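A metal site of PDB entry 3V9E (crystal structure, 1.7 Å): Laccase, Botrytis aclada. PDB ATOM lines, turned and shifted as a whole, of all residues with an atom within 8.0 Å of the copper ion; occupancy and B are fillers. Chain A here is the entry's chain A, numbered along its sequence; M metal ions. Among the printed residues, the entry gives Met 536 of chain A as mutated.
The side-chain sulfur (SG) of Cys 526 lies close to the backbone NH (N) of Ile 528 (3.4 Å). The side-chain sulfur of Met 536 lies close to a ring nitrogen (ND1) of His 463. The backbone NH of Cys 526 sits at hydrogen-bond distance from the backbone carbonyl oxygen of Met 536. The backbone carbonyl oxygen of His 463 sits at hydrogen-bond distance from the backbone NH of Leu 504 (2.8 Å). The backbone carbonyl oxygen of His 531 sits at hydrogen-bond distance from the backbone NH of Met 536, at 2.9 Å.
CD1 of Ile 528 touches the copper ion, at 3.7 Å. SD of Met 536 touches the copper ion (3.2 Å). Five residues have an atom within 4 Å of the copper ion: His 463, Cys 526, Ile 528, His 531 and Met 536.
The copper ion is bound by a ring nitrogen (ND1) of His 463 (2.0 Å), a ring nitrogen (ND1) of His 531 (2.0 Å) and the side-chain sulfur of Cys 526 (2.2 Å). The copper ion has three donor atoms within binding distance.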
ATOM      1  N   ASP A 273      22.103   3.510  -3.688  1.00  0.00           N
ATOM      2  CA  ASP A 273      21.070   4.544  -4.029  1.00  0.00           C
ATOM      3  C   ASP A 273      21.736   5.891  -4.237  1.00  0.00           C
ATOM      4  O   ASP A 273      21.587   6.837  -3.462  1.00  0.00           O
ATOM      5  CB  ASP A 273      19.992   4.567  -2.900  1.00  0.00           C
ATOM      6  CG  ASP A 273      18.745   5.379  -3.287  1.00  0.00           C
ATOM      7  OD1 ASP A 273      18.685   5.908  -4.391  1.00  0.00           O
ATOM      8  OD2 ASP A 273      17.836   5.541  -2.475  1.00  0.00           O
ATOM      9  N   ILE A 307      22.866   3.914 -11.408  1.00  0.00           N
ATOM     10  CA  ILE A 307      23.405   2.752 -10.718  1.00  0.00           C
ATOM     11  C   ILE A 307      23.476   1.543 -11.666  1.00  0.00           C
ATOM     12  O   ILE A 307      22.482   1.136 -12.280  1.00  0.00           O
ATOM     13  CB  ILE A 307      22.553   2.333  -9.518  1.00  0.00           C
ATOM     14  CG1 ILE A 307      22.567   3.421  -8.455  1.00  0.00           C
ATOM     15  CG2 ILE A 307      23.172   1.068  -8.919  1.00  0.00           C
ATOM     16  CD1 ILE A 307      21.534   3.121  -7.422  1.00  0.00           C
ATOM     17  N   VAL A 394       4.643   0.385 -13.011  1.00  0.00           N
ATOM     18  CA  VAL A 394       5.161   0.433 -11.668  1.00  0.00           C
ATOM     19  C   VAL A 394       4.302   1.315 -10.768  1.00  0.00           C
ATOM     20  O   VAL A 394       4.039   2.505 -11.087  1.00  0.00           O
ATOM     21  CB  VAL A 394       6.556   1.028 -11.623  1.00  0.00           C
ATOM     22  CG1 VAL A 394       7.104   0.935 -10.198  1.00  0.00           C
ATOM     23  CG2 VAL A 394       7.503   0.297 -12.557  1.00  0.00           C
ATOM     24  N   TRP A 404       7.269  -2.156  -4.022  1.00  0.00           N
ATOM     25  CA  TRP A 404       7.006  -1.678  -5.354  1.00  0.00           C
ATOM     26  C   TRP A 404       6.322  -2.787  -6.059  1.00  0.00           C
ATOM     27  O   TRP A 404       6.645  -3.979  -5.876  1.00  0.00           O
ATOM     28  CB  TRP A 404       8.302  -1.312  -6.139  1.00  0.00           C
ATOM     29  CG  TRP A 404       9.129  -0.332  -5.427  1.00  0.00           C
ATOM     30  CD1 TRP A 404      10.033  -0.621  -4.522  1.00  0.00           C
ATOM     31  CD2 TRP A 404       9.127   1.074  -5.563  1.00  0.00           C
ATOM     32  NE1 TRP A 404      10.550   0.475  -3.973  1.00  0.00           N
ATOM     33  CE2 TRP A 404      10.037   1.571  -4.624  1.00  0.00           C
ATOM     34  CE3 TRP A 404       8.417   1.980  -6.347  1.00  0.00           C
ATOM     35  CZ2 TRP A 404      10.291   2.898  -4.468  1.00  0.00           C
ATOM     36  CZ3 TRP A 404       8.665   3.298  -6.172  1.00  0.00           C
ATOM     37  CH2 TRP A 404       9.606   3.760  -5.261  1.00  0.00           C
ATOM     38  N   ILE A 461      11.201   9.605  -9.190  1.00  0.00           N
ATOM     39  CA  ILE A 461      12.524   8.962  -9.100  1.00  0.00           C
ATOM     40  C   ILE A 461      12.894   8.434 -10.511  1.00  0.00           C
ATOM     41  O   ILE A 461      12.055   7.847 -11.178  1.00  0.00           O
ATOM     42  CB  ILE A 461      12.496   7.807  -8.103  1.00  0.00           C
ATOM     43  CG1 ILE A 461      12.306   8.298  -6.661  1.00  0.00           C
ATOM     44  CG2 ILE A 461      13.815   7.087  -8.165  1.00  0.00           C
ATOM     45  CD1 ILE A 461      11.792   7.208  -5.732  1.00  0.00           C
ATOM     46  N   TRP A 462      14.149   8.575 -10.893  1.00  0.00           N
ATOM     47  CA  TRP A 462      14.640   8.012 -12.150  1.00  0.00           C
ATOM     48  C   TRP A 462      15.310   6.661 -11.832  1.00  0.00           C
ATOM     49  O   TRP A 462      16.404   6.635 -11.263  1.00  0.00           O
ATOM     50  CB  TRP A 462      15.632   8.981 -12.739  1.00  0.00           C
ATOM     51  CG  TRP A 462      14.955  10.175 -13.346  1.00  0.00           C
ATOM     52  CD1 TRP A 462      14.224  11.103 -12.708  1.00  0.00           C
ATOM     53  CD2 TRP A 462      14.978  10.568 -14.754  1.00  0.00           C
ATOM     54  NE1 TRP A 462      13.794  12.077 -13.582  1.00  0.00           N
ATOM     55  CE2 TRP A 462      14.177  11.725 -14.866  1.00  0.00           C
ATOM     56  CE3 TRP A 462      15.514   9.992 -15.919  1.00  0.00           C
ATOM     57  CZ2 TRP A 462      14.027  12.406 -16.057  1.00  0.00           C
ATOM     58  CZ3 TRP A 462      15.321  10.650 -17.136  1.00  0.00           C
ATOM     59  CH2 TRP A 462      14.584  11.833 -17.199  1.00  0.00           C
ATOM     60  N   HIS A 463      14.610   5.564 -12.118  1.00  0.00           N
ATOM     61  CA  HIS A 463      14.989   4.283 -11.591  1.00  0.00           C
ATOM     62  C   HIS A 463      15.900   3.615 -12.594  1.00  0.00           C
ATOM     63  O   HIS A 463      15.482   3.387 -13.717  1.00  0.00           O
ATOM     64  CB  HIS A 463      13.757   3.378 -11.447  1.00  0.00           C
ATOM     65  CG  HIS A 463      12.713   3.911 -10.516  1.00  0.00           C
ATOM     66  ND1 HIS A 463      12.562   3.465  -9.207  1.00  0.00           N
ATOM     67  CD2 HIS A 463      11.712   4.813 -10.730  1.00  0.00           C
ATOM     68  CE1 HIS A 463      11.546   4.116  -8.634  1.00  0.00           C
ATOM     69  NE2 HIS A 463      10.990   4.872  -9.559  1.00  0.00           N
ATOM     70  N   PRO A 464      17.131   3.227 -12.198  1.00  0.00           N
ATOM     71  CA  PRO A 464      18.020   2.488 -13.092  1.00  0.00           C
ATOM     72  C   PRO A 464      17.575   1.070 -13.341  1.00  0.00           C
ATOM     73  O   PRO A 464      17.616   0.242 -12.432  1.00  0.00           O
ATOM     74  CB  PRO A 464      19.352   2.458 -12.353  1.00  0.00           C
ATOM     75  CG  PRO A 464      18.969   2.579 -10.891  1.00  0.00           C
ATOM     76  CD  PRO A 464      17.698   3.408 -10.843  1.00  0.00           C
ATOM     77  N   ILE A 465      17.086   0.798 -14.539  1.00  0.00           N
ATOM     78  CA  ILE A 465      16.500  -0.500 -14.817  1.00  0.00           C
ATOM     79  C   ILE A 465      17.556  -1.360 -15.522  1.00  0.00           C
ATOM     80  O   ILE A 465      18.100  -0.959 -16.588  1.00  0.00           O
ATOM     81  CB  ILE A 465      15.295  -0.362 -15.771  1.00  0.00           C
ATOM     82  CG1 ILE A 465      14.225   0.570 -15.153  1.00  0.00           C
ATOM     83  CG2 ILE A 465      14.768  -1.733 -16.192  1.00  0.00           C
ATOM     84  CD1 ILE A 465      13.626   0.071 -13.833  1.00  0.00           C
ATOM     85  N   LEU A 504      14.355   4.430 -16.002  1.00  0.00           N
ATOM     86  CA  LEU A 504      12.936   4.736 -16.107  1.00  0.00           C
ATOM     87  C   LEU A 504      12.700   6.148 -15.562  1.00  0.00           C
ATOM     88  O   LEU A 504      12.931   6.389 -14.368  1.00  0.00           O
ATOM     89  CB  LEU A 504      12.144   3.776 -15.317  1.00  0.00           C
ATOM     90  CG  LEU A 504      10.717   4.165 -14.953  1.00  0.00           C
ATOM     91  CD1 LEU A 504       9.924   4.315 -16.228  1.00  0.00           C
ATOM     92  CD2 LEU A 504      10.134   3.040 -14.054  1.00  0.00           C
ATOM     93  N   HIS A 525      14.970  -5.415 -13.266  1.00  0.00           N
ATOM     94  CA  HIS A 525      14.761  -4.784 -12.012  1.00  0.00           C
ATOM     95  C   HIS A 525      15.391  -3.456 -11.900  1.00  0.00           C
ATOM     96  O   HIS A 525      16.350  -3.129 -12.598  1.00  0.00           O
ATOM     97  CB  HIS A 525      15.307  -5.683 -10.892  1.00  0.00           C
ATOM     98  CG  HIS A 525      16.801  -5.856 -10.954  1.00  0.00           C
ATOM     99  ND1 HIS A 525      17.629  -5.140 -10.112  1.00  0.00           N
ATOM    100  CD2 HIS A 525      17.600  -6.619 -11.732  1.00  0.00           C
ATOM    101  CE1 HIS A 525      18.893  -5.497 -10.366  1.00  0.00           C
ATOM    102  NE2 HIS A 525      18.896  -6.382 -11.354  1.00  0.00           N
ATOM    103  N   CYS A 526      14.882  -2.690 -10.936  1.00  0.00           N
ATOM    104  CA  CYS A 526      15.485  -1.470 -10.521  1.00  0.00           C
ATOM    105  C   CYS A 526      16.757  -1.820  -9.765  1.00  0.00           C
ATOM    106  O   CYS A 526      16.705  -2.707  -8.898  1.00  0.00           O
ATOM    107  CB  CYS A 526      14.578  -0.652  -9.612  1.00  0.00           C
ATOM    108  SG  CYS A 526      15.359   0.914  -9.171  1.00  0.00           S
ATOM    109  N   HIS A 527      17.819  -1.068 -10.013  1.00  0.00           N
ATOM    110  CA  HIS A 527      19.145  -1.381  -9.407  1.00  0.00           C
ATOM    111  C   HIS A 527      19.368  -0.556  -8.167  1.00  0.00           C
ATOM    112  O   HIS A 527      20.392  -0.704  -7.550  1.00  0.00           O
ATOM    113  CB  HIS A 527      20.287  -1.142 -10.442  1.00  0.00           C
ATOM    114  CG  HIS A 527      21.433  -2.105 -10.352  1.00  0.00           C
ATOM    115  ND1 HIS A 527      22.188  -2.270  -9.210  1.00  0.00           N
ATOM    116  CD2 HIS A 527      21.991  -2.925 -11.296  1.00  0.00           C
ATOM    117  CE1 HIS A 527      23.163  -3.136  -9.436  1.00  0.00           C
ATOM    118  NE2 HIS A 527      23.060  -3.566 -10.700  1.00  0.00           N
ATOM    119  N   ILE A 528      18.417   0.294  -7.786  1.00  0.00           N
ATOM    120  CA  ILE A 528      18.487   0.957  -6.492  1.00  0.00           C
ATOM    121  C   ILE A 528      18.225  -0.189  -5.505  1.00  0.00           C
ATOM    122  O   ILE A 528      17.229  -0.891  -5.585  1.00  0.00           O
ATOM    123  CB  ILE A 528      17.452   2.078  -6.356  1.00  0.00           C
ATOM    124  CG1 ILE A 528      17.806   3.245  -7.258  1.00  0.00           C
ATOM    125  CG2 ILE A 528      17.381   2.466  -4.866  1.00  0.00           C
ATOM    126  CD1 ILE A 528      16.636   4.234  -7.395  1.00  0.00           C
ATOM    127  N   ALA A 529      19.209  -0.485  -4.672  1.00  0.00           N
ATOM    128  CA  ALA A 529      19.151  -1.769  -3.938  1.00  0.00           C
ATOM    129  C   ALA A 529      17.899  -1.889  -3.077  1.00  0.00           C
ATOM    130  O   ALA A 529      17.291  -2.990  -2.966  1.00  0.00           O
ATOM    131  CB  ALA A 529      20.418  -1.900  -3.076  1.00  0.00           C
ATOM    132  N   TRP A 530      17.515  -0.785  -2.442  1.00  0.00           N
ATOM    133  CA  TRP A 530      16.287  -0.788  -1.623  1.00  0.00           C
ATOM    134  C   TRP A 530      15.072  -1.211  -2.446  1.00  0.00           C
ATOM    135  O   TRP A 530      14.242  -1.984  -1.967  1.00  0.00           O
ATOM    136  CB  TRP A 530      16.064   0.546  -0.964  1.00  0.00           C
ATOM    137  CG  TRP A 530      17.267   1.145  -0.238  1.00  0.00           C
ATOM    138  CD1 TRP A 530      17.841   2.282  -0.508  1.00  0.00           C
ATOM    139  CD2 TRP A 530      17.938   0.593   0.915  1.00  0.00           C
ATOM    140  NE1 TRP A 530      18.822   2.563   0.434  1.00  0.00           N
ATOM    141  CE2 TRP A 530      18.884   1.506   1.307  1.00  0.00           C
ATOM    142  CE3 TRP A 530      17.789  -0.569   1.663  1.00  0.00           C
ATOM    143  CZ2 TRP A 530      19.744   1.282   2.410  1.00  0.00           C
ATOM    144  CZ3 TRP A 530      18.606  -0.757   2.802  1.00  0.00           C
ATOM    145  CH2 TRP A 530      19.581   0.154   3.115  1.00  0.00           C
ATOM    146  N   HIS A 531      14.984  -0.693  -3.652  1.00  0.00           N
ATOM    147  CA  HIS A 531      13.828  -0.893  -4.511  1.00  0.00           C
ATOM    148  C   HIS A 531      13.826  -2.297  -5.000  1.00  0.00           C
ATOM    149  O   HIS A 531      12.790  -2.945  -5.041  1.00  0.00           O
ATOM    150  CB  HIS A 531      13.846   0.063  -5.740  1.00  0.00           C
ATOM    151  CG  HIS A 531      13.717   1.485  -5.379  1.00  0.00           C
ATOM    152  ND1 HIS A 531      13.587   2.472  -6.317  1.00  0.00           N
ATOM    153  CD2 HIS A 531      13.802   2.121  -4.170  1.00  0.00           C
ATOM    154  CE1 HIS A 531      13.505   3.641  -5.708  1.00  0.00           C
ATOM    155  NE2 HIS A 531      13.670   3.456  -4.408  1.00  0.00           N
ATOM    156  N   ALA A 532      14.979  -2.849  -5.350  1.00  0.00           N
ATOM    157  CA  ALA A 532      15.046  -4.249  -5.708  1.00  0.00           C
ATOM    158  C   ALA A 532      14.587  -5.160  -4.579  1.00  0.00           C
ATOM    159  O   ALA A 532      13.840  -6.112  -4.737  1.00  0.00           O
ATOM    160  CB  ALA A 532      16.487  -4.598  -6.136  1.00  0.00           C
ATOM    161  N   GLU A 534      12.651  -4.322  -2.232  1.00  0.00           N
ATOM    162  CA  GLU A 534      11.252  -3.971  -2.068  1.00  0.00           C
ATOM    163  C   GLU A 534      10.421  -4.492  -3.234  1.00  0.00           C
ATOM    164  O   GLU A 534       9.278  -4.073  -3.384  1.00  0.00           O
ATOM    165  CB  GLU A 534      11.089  -2.496  -1.885  1.00  0.00           C
ATOM    166  CG  GLU A 534      11.693  -2.075  -0.549  1.00  0.00           C
ATOM    167  CD  GLU A 534      12.042  -0.678  -0.407  1.00  0.00           C
ATOM    168  OE1 GLU A 534      11.773   0.111  -1.335  1.00  0.00           O
ATOM    169  OE2 GLU A 534      12.600  -0.333   0.691  1.00  0.00           O
ATOM    170  N   MET A 536      10.857  -4.235  -6.769  1.00  0.00           N
ATOM    171  CA  MET A 536      10.735  -3.531  -8.012  1.00  0.00           C
ATOM    172  C   MET A 536      11.428  -4.344  -9.118  1.00  0.00           C
ATOM    173  O   MET A 536      12.530  -4.035  -9.543  1.00  0.00           O
ATOM    174  CB  MET A 536      11.276  -2.114  -7.935  1.00  0.00           C
ATOM    175  CG  MET A 536      10.816  -1.356  -9.146  1.00  0.00           C
ATOM    176  SD  MET A 536      11.152   0.388  -8.938  1.00  0.00           S
ATOM    177  CE  MET A 536      11.059   0.901 -10.642  1.00  0.00           C
HETATM  178 CU    CU M   1      13.750   2.133  -8.300  1.00  0.00          CU
